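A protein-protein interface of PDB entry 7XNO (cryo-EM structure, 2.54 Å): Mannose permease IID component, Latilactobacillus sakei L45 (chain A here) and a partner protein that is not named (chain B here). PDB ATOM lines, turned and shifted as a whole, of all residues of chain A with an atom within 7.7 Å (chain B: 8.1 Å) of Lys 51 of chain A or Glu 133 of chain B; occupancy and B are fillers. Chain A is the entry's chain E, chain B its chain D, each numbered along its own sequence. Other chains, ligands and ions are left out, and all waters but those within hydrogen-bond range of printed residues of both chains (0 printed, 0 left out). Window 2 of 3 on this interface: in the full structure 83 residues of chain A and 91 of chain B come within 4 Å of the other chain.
The backbone carbonyl oxygen (O) of Ala 131 of chain B lies within hydrogen-bond range of the side-chain hydroxyl (OG) of Ser 55 of chain A (3.1 Å). The side-chain hydroxyl of Ser 55 of chain A is in hydrogen-bond range of the backbone carbonyl oxygen of Lys 132 of chain B (3.0 Å). The side-chain amino group of Lys 51 of chain A lies within salt-bridge range of the side-chain carboxylate of Glu 133 of chain B (3.1 Å).
The backbone NH of Asn 135 of chain B sits at hydrogen-bond distance from the backbone carbonyl oxygen of Ala 130 of chain B (3.3 Å). The backbone carbonyl oxygen (O) of Tyr 48 of chain A sits close to the guanidinium group (NH1) of Arg 54 of chain A.
Among the printed residues, pairs that only touch across the chains: Arg 54 of chain A with Phe 136 of chain B (3.2 Å), Leu 58 of chain A with Phe 136 of chain B (3.5 Å), Leu 58 of chain A with Gly 134 of chain B (3.6 Å), Leu 58 of chain A with Ala 131 of chain B (3.6 Å), Val 59 of chain A with Ala 131 of chain B (3.7 Å), Val 59 of chain A with Lys 132 of chain B (3.7 Å), Leu 58 of chain A with Ile 139 of chain B (3.7 Å), Ser 55 of chain A with Gly 134 of chain B (3.8 Å) and Leu 58 of chain A with Asn 135 of chain B (3.97 Å).
Lys 51 of chain A touches just one residue of chain B: Glu 133. Printed residues of chain A within 4 Å of Glu 133 of chain B: Lys 51. No residue of chain B comes within 4 Å of Thr 50 of chain A. Printed residues of chain A within 4 Å of Ala 131 of chain B: Ser 55 (3.1 Å), Leu 58 (3.6 Å) and Val 59 (3.7 Å). Of the printed residues of chain B, Val 59 of chain A touches Ala 131 and Lys 132. Of the printed residues of chain B, Leu 58 of chain A touches Ala 131, Gly 134, Asn 135, Phe 136 and Ile 139. Printed residues of chain A within 4 Å of Lys 132 of chain B: Ser 55 (3.0 Å) and Val 59 (3.7 Å). Of the printed residues of chain A, Asn 135 of chain B touches Leu 58 (3.97 Å). Ala 56 of chain A touches none of the printed residues of chain B. The nearest residue of chain B that does not touch Lys 51 of chain A is Gly 134 of chain B (5.2 Å). The nearest residue of chain A that does not touch Glu 133 of chain B is Ser 55 of chain A (4.03 Å).
Of the 12 printed residues of chain B, 7 touch a printed residue of chain A. Printed residues of chain B that touch a printed residue of chain A: Ala 131, Lys 132, Glu 133, Gly 134, Asn 135, Phe 136 and Ile 139. Hydrophobic or aromatic side chains of chain B that line the printed part of chain A: Ala 131, Phe 136 and Ile 139. Of the 11 printed residues of chain A, 5 touch a printed residue of chain B. Among the printed residues, Asp or Glu carboxylates within 4 Å of a Lys or Arg side-chain nitrogen of the other chain: Lys 51 of chain A with Glu 133 of chain B (3.1 Å).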
ATOM      1  N   TYR A  48     -15.605  12.957  26.577  1.00  0.00           N
ATOM      2  CA  TYR A  48     -16.390  12.262  25.568  1.00  0.00           C
ATOM      3  C   TYR A  48     -15.551  11.182  24.899  1.00  0.00           C
ATOM      4  O   TYR A  48     -14.353  11.368  24.671  1.00  0.00           O
ATOM      5  CB  TYR A  48     -16.916  13.248  24.523  1.00  0.00           C
ATOM      6  CG  TYR A  48     -17.718  14.383  25.119  1.00  0.00           C
ATOM      7  CD1 TYR A  48     -18.986  14.167  25.638  1.00  0.00           C
ATOM      8  CD2 TYR A  48     -17.205  15.671  25.165  1.00  0.00           C
ATOM      9  CE1 TYR A  48     -19.721  15.199  26.183  1.00  0.00           C
ATOM     10  CE2 TYR A  48     -17.932  16.711  25.709  1.00  0.00           C
ATOM     11  CZ  TYR A  48     -19.190  16.468  26.217  1.00  0.00           C
ATOM     12  OH  TYR A  48     -19.920  17.499  26.760  1.00  0.00           O
ATOM     13  N   LYS A  49     -16.184  10.048  24.594  1.00  0.00           N
ATOM     14  CA  LYS A  49     -15.467   8.906  24.029  1.00  0.00           C
ATOM     15  C   LYS A  49     -16.151   8.228  22.850  1.00  0.00           C
ATOM     16  O   LYS A  49     -15.463   7.533  22.095  1.00  0.00           O
ATOM     17  CB  LYS A  49     -15.213   7.851  25.113  1.00  0.00           C
ATOM     18  CG  LYS A  49     -13.853   7.952  25.773  1.00  0.00           C
ATOM     19  CD  LYS A  49     -13.919   8.776  27.045  1.00  0.00           C
ATOM     20  CE  LYS A  49     -12.582   8.778  27.765  1.00  0.00           C
ATOM     21  NZ  LYS A  49     -12.624   9.590  29.009  1.00  0.00           N
ATOM     22  N   THR A  50     -17.458   8.392  22.647  1.00  0.00           N
ATOM     23  CA  THR A  50     -18.201   7.514  21.749  1.00  0.00           C
ATOM     24  C   THR A  50     -18.003   7.828  20.270  1.00  0.00           C
ATOM     25  O   THR A  50     -18.498   7.065  19.433  1.00  0.00           O
ATOM     26  CB  THR A  50     -19.694   7.565  22.078  1.00  0.00           C
ATOM     27  OG1 THR A  50     -20.405   6.664  21.219  1.00  0.00           O
ATOM     28  CG2 THR A  50     -20.234   8.968  21.884  1.00  0.00           C
ATOM     29  N   LYS A  51     -17.300   8.908  19.932  1.00  0.00           N
ATOM     30  CA  LYS A  51     -17.017   9.418  18.592  1.00  0.00           C
ATOM     31  C   LYS A  51     -18.225  10.127  17.976  1.00  0.00           C
ATOM     32  O   LYS A  51     -18.078  10.763  16.931  1.00  0.00           O
ATOM     33  CB  LYS A  51     -16.518   8.329  17.618  1.00  0.00           C
ATOM     34  CG  LYS A  51     -15.783   8.841  16.385  1.00  0.00           C
ATOM     35  CD  LYS A  51     -16.596   8.590  15.124  1.00  0.00           C
ATOM     36  CE  LYS A  51     -15.808   8.926  13.869  1.00  0.00           C
ATOM     37  NZ  LYS A  51     -16.614   8.708  12.637  1.00  0.00           N
ATOM     38  N   GLU A  52     -19.406  10.071  18.592  1.00  0.00           N
ATOM     39  CA  GLU A  52     -20.474  11.005  18.258  1.00  0.00           C
ATOM     40  C   GLU A  52     -20.540  12.173  19.226  1.00  0.00           C
ATOM     41  O   GLU A  52     -20.880  13.287  18.816  1.00  0.00           O
ATOM     42  CB  GLU A  52     -21.838  10.304  18.228  1.00  0.00           C
ATOM     43  CG  GLU A  52     -22.015   9.286  17.108  1.00  0.00           C
ATOM     44  CD  GLU A  52     -21.431   7.932  17.440  1.00  0.00           C
ATOM     45  OE1 GLU A  52     -20.941   7.759  18.573  1.00  0.00           O
ATOM     46  OE2 GLU A  52     -21.463   7.038  16.568  1.00  0.00           O
ATOM     47  N   ASP A  53     -20.224  11.937  20.500  1.00  0.00           N
ATOM     48  CA  ASP A  53     -20.090  13.035  21.449  1.00  0.00           C
ATOM     49  C   ASP A  53     -18.867  13.884  21.132  1.00  0.00           C
ATOM     50  O   ASP A  53     -18.900  15.111  21.282  1.00  0.00           O
ATOM     51  CB  ASP A  53     -20.010  12.484  22.872  1.00  0.00           C
ATOM     52  CG  ASP A  53     -21.367  12.097  23.426  1.00  0.00           C
ATOM     53  OD1 ASP A  53     -22.388  12.604  22.918  1.00  0.00           O
ATOM     54  OD2 ASP A  53     -21.411  11.284  24.372  1.00  0.00           O
ATOM     55  N   ARG A  54     -17.776  13.248  20.695  1.00  0.00           N
ATOM     56  CA  ARG A  54     -16.586  13.991  20.288  1.00  0.00           C
ATOM     57  C   ARG A  54     -16.898  14.927  19.127  1.00  0.00           C
ATOM     58  O   ARG A  54     -16.589  16.124  19.174  1.00  0.00           O
ATOM     59  CB  ARG A  54     -15.474  13.019  19.891  1.00  0.00           C
ATOM     60  CG  ARG A  54     -14.772  12.309  21.035  1.00  0.00           C
ATOM     61  CD  ARG A  54     -13.705  11.372  20.478  1.00  0.00           C
ATOM     62  NE  ARG A  54     -13.246  10.383  21.448  1.00  0.00           N
ATOM     63  CZ  ARG A  54     -12.442  10.644  22.468  1.00  0.00           C
ATOM     64  NH1 ARG A  54     -11.974  11.862  22.686  1.00  0.00           N
ATOM     65  NH2 ARG A  54     -12.095   9.658  23.289  1.00  0.00           N
ATOM     66  N   SER A  55     -17.510  14.388  18.069  1.00  0.00           N
ATOM     67  CA  SER A  55     -17.839  15.197  16.901  1.00  0.00           C
ATOM     68  C   SER A  55     -18.842  16.288  17.250  1.00  0.00           C
ATOM     69  O   SER A  55     -18.718  17.427  16.784  1.00  0.00           O
ATOM     70  CB  SER A  55     -18.383  14.305  15.785  1.00  0.00           C
ATOM     71  OG  SER A  55     -18.755  15.071  14.654  1.00  0.00           O
ATOM     72  N   ALA A  56     -19.851  15.954  18.058  1.00  0.00           N
ATOM     73  CA  ALA A  56     -20.841  16.949  18.450  1.00  0.00           C
ATOM     74  C   ALA A  56     -20.199  18.082  19.238  1.00  0.00           C
ATOM     75  O   ALA A  56     -20.492  19.257  18.996  1.00  0.00           O
ATOM     76  CB  ALA A  56     -21.957  16.293  19.262  1.00  0.00           C
ATOM     77  N   LEU A  58     -17.024  19.017  19.125  1.00  0.00           N
ATOM     78  CA  LEU A  58     -16.158  19.776  18.229  1.00  0.00           C
ATOM     79  C   LEU A  58     -16.964  20.743  17.371  1.00  0.00           C
ATOM     80  O   LEU A  58     -16.599  21.916  17.232  1.00  0.00           O
ATOM     81  CB  LEU A  58     -15.343  18.824  17.354  1.00  0.00           C
ATOM     82  CG  LEU A  58     -14.083  18.252  18.002  1.00  0.00           C
ATOM     83  CD1 LEU A  58     -13.383  17.291  17.059  1.00  0.00           C
ATOM     84  CD2 LEU A  58     -13.147  19.373  18.425  1.00  0.00           C
ATOM     85  N   VAL A  59     -18.074  20.273  16.797  1.00  0.00           N
ATOM     86  CA  VAL A  59     -18.917  21.151  15.989  1.00  0.00           C
ATOM     87  C   VAL A  59     -19.530  22.244  16.856  1.00  0.00           C
ATOM     88  O   VAL A  59     -19.695  23.389  16.418  1.00  0.00           O
ATOM     89  CB  VAL A  59     -19.995  20.331  15.255  1.00  0.00           C
ATOM     90  CG1 VAL A  59     -20.937  21.246  14.490  1.00  0.00           C
ATOM     91  CG2 VAL A  59     -19.348  19.334  14.313  1.00  0.00           C
ATOM     92  N   MET B 127     -10.694  22.702   9.131  1.00  0.00           N
ATOM     93  CA  MET B 127     -10.866  22.288  10.519  1.00  0.00           C
ATOM     94  C   MET B 127     -12.323  21.964  10.831  1.00  0.00           C
ATOM     95  O   MET B 127     -12.594  21.080  11.647  1.00  0.00           O
ATOM     96  CB  MET B 127     -10.344  23.372  11.458  1.00  0.00           C
ATOM     97  CG  MET B 127      -8.831  23.414  11.551  1.00  0.00           C
ATOM     98  SD  MET B 127      -8.205  24.917  12.317  1.00  0.00           S
ATOM     99  CE  MET B 127      -8.818  24.720  13.983  1.00  0.00           C
ATOM    100  N   ASP B 128     -13.266  22.668  10.204  1.00  0.00           N
ATOM    101  CA  ASP B 128     -14.675  22.306  10.333  1.00  0.00           C
ATOM    102  C   ASP B 128     -14.939  20.922   9.758  1.00  0.00           C
ATOM    103  O   ASP B 128     -15.661  20.113  10.356  1.00  0.00           O
ATOM    104  CB  ASP B 128     -15.552  23.341   9.629  1.00  0.00           C
ATOM    105  CG  ASP B 128     -15.919  24.500  10.524  1.00  0.00           C
ATOM    106  OD1 ASP B 128     -16.442  24.257  11.632  1.00  0.00           O
ATOM    107  OD2 ASP B 128     -15.689  25.656  10.117  1.00  0.00           O
ATOM    108  N   ALA B 129     -14.369  20.638   8.586  1.00  0.00           N
ATOM    109  CA  ALA B 129     -14.517  19.311   7.998  1.00  0.00           C
ATOM    110  C   ALA B 129     -13.934  18.241   8.913  1.00  0.00           C
ATOM    111  O   ALA B 129     -14.484  17.140   9.027  1.00  0.00           O
ATOM    112  CB  ALA B 129     -13.855  19.264   6.622  1.00  0.00           C
ATOM    113  N   ALA B 130     -12.811  18.548   9.566  1.00  0.00           N
ATOM    114  CA  ALA B 130     -12.233  17.619  10.535  1.00  0.00           C
ATOM    115  C   ALA B 130     -13.141  17.436  11.745  1.00  0.00           C
ATOM    116  O   ALA B 130     -13.319  16.314  12.232  1.00  0.00           O
ATOM    117  CB  ALA B 130     -10.854  18.111  10.973  1.00  0.00           C
ATOM    118  N   ALA B 131     -13.714  18.531  12.249  1.00  0.00           N
ATOM    119  CA  ALA B 131     -14.586  18.465  13.417  1.00  0.00           C
ATOM    120  C   ALA B 131     -15.851  17.672  13.131  1.00  0.00           C
ATOM    121  O   ALA B 131     -16.419  17.064  14.046  1.00  0.00           O
ATOM    122  CB  ALA B 131     -14.941  19.875  13.887  1.00  0.00           C
ATOM    123  N   LYS B 132     -16.312  17.670  11.878  1.00  0.00           N
ATOM    124  CA  LYS B 132     -17.465  16.847  11.528  1.00  0.00           C
ATOM    125  C   LYS B 132     -17.184  15.359  11.697  1.00  0.00           C
ATOM    126  O   LYS B 132     -18.127  14.563  11.733  1.00  0.00           O
ATOM    127  CB  LYS B 132     -17.911  17.126  10.091  1.00  0.00           C
ATOM    128  CG  LYS B 132     -18.324  18.562   9.837  1.00  0.00           C
ATOM    129  CD  LYS B 132     -19.571  18.928  10.620  1.00  0.00           C
ATOM    130  CE  LYS B 132     -20.073  20.306  10.234  1.00  0.00           C
ATOM    131  NZ  LYS B 132     -19.145  21.377  10.694  1.00  0.00           N
ATOM    132  N   GLU B 133     -15.914  14.968  11.797  1.00  0.00           N
ATOM    133  CA  GLU B 133     -15.535  13.578  12.006  1.00  0.00           C
ATOM    134  C   GLU B 133     -15.000  13.307  13.405  1.00  0.00           C
ATOM    135  O   GLU B 133     -14.659  12.158  13.709  1.00  0.00           O
ATOM    136  CB  GLU B 133     -14.489  13.154  10.968  1.00  0.00           C
ATOM    137  CG  GLU B 133     -15.057  12.878   9.587  1.00  0.00           C
ATOM    138  CD  GLU B 133     -15.507  11.440   9.417  1.00  0.00           C
ATOM    139  OE1 GLU B 133     -15.728  11.017   8.263  1.00  0.00           O
ATOM    140  OE2 GLU B 133     -15.640  10.730  10.437  1.00  0.00           O
ATOM    141  N   GLY B 134     -14.920  14.321  14.263  1.00  0.00           N
ATOM    142  CA  GLY B 134     -14.377  14.118  15.592  1.00  0.00           C
ATOM    143  C   GLY B 134     -12.881  13.920  15.640  1.00  0.00           C
ATOM    144  O   GLY B 134     -12.375  13.329  16.597  1.00  0.00           O
ATOM    145  N   ASN B 135     -12.154  14.400  14.633  1.00  0.00           N
ATOM    146  CA  ASN B 135     -10.712  14.202  14.539  1.00  0.00           C
ATOM    147  C   ASN B 135     -10.002  15.343  15.259  1.00  0.00           C
ATOM    148  O   ASN B 135      -9.956  16.471  14.757  1.00  0.00           O
ATOM    149  CB  ASN B 135     -10.280  14.120  13.078  1.00  0.00           C
ATOM    150  CG  ASN B 135      -8.980  13.365  12.896  1.00  0.00           C
ATOM    151  OD1 ASN B 135      -8.252  13.119  13.857  1.00  0.00           O
ATOM    152  ND2 ASN B 135      -8.682  12.991  11.658  1.00  0.00           N
ATOM    153  N   PHE B 136      -9.451  15.051  16.439  1.00  0.00           N
ATOM    154  CA  PHE B 136      -8.692  16.057  17.175  1.00  0.00           C
ATOM    155  C   PHE B 136      -7.326  16.290  16.542  1.00  0.00           C
ATOM    156  O   PHE B 136      -6.827  17.424  16.521  1.00  0.00           O
ATOM    157  CB  PHE B 136      -8.531  15.626  18.632  1.00  0.00           C
ATOM    158  CG  PHE B 136      -9.821  15.568  19.398  1.00  0.00           C
ATOM    159  CD1 PHE B 136     -10.617  16.691  19.531  1.00  0.00           C
ATOM    160  CD2 PHE B 136     -10.234  14.387  19.988  1.00  0.00           C
ATOM    161  CE1 PHE B 136     -11.800  16.637  20.240  1.00  0.00           C
ATOM    162  CE2 PHE B 136     -11.417  14.328  20.694  1.00  0.00           C
ATOM    163  CZ  PHE B 136     -12.200  15.453  20.820  1.00  0.00           C
ATOM    164  N   LYS B 138      -6.302  16.163  13.390  1.00  0.00           N
ATOM    165  CA  LYS B 138      -6.334  17.026  12.214  1.00  0.00           C
ATOM    166  C   LYS B 138      -6.544  18.486  12.599  1.00  0.00           C
ATOM    167  O   LYS B 138      -5.923  19.385  12.017  1.00  0.00           O
ATOM    168  CB  LYS B 138      -7.423  16.554  11.253  1.00  0.00           C
ATOM    169  CG  LYS B 138      -7.355  17.182   9.872  1.00  0.00           C
ATOM    170  CD  LYS B 138      -8.359  16.542   8.927  1.00  0.00           C
ATOM    171  CE  LYS B 138      -8.577  17.399   7.692  1.00  0.00           C
ATOM    172  NZ  LYS B 138      -9.754  16.945   6.898  1.00  0.00           N
ATOM    173  N   ILE B 139      -7.415  18.743  13.578  1.00  0.00           N
ATOM    174  CA  ILE B 139      -7.650  20.113  14.025  1.00  0.00           C
ATOM    175  C   ILE B 139      -6.384  20.702  14.633  1.00  0.00           C
ATOM    176  O   ILE B 139      -6.016  21.850  14.350  1.00  0.00           O
ATOM    177  CB  ILE B 139      -8.832  20.156  15.012  1.00  0.00           C
ATOM    178  CG1 ILE B 139     -10.150  19.952  14.267  1.00  0.00           C
ATOM    179  CG2 ILE B 139      -8.852  21.468  15.779  1.00  0.00           C
ATOM    180  CD1 ILE B 139     -11.344  19.804  15.174  1.00  0.00           C
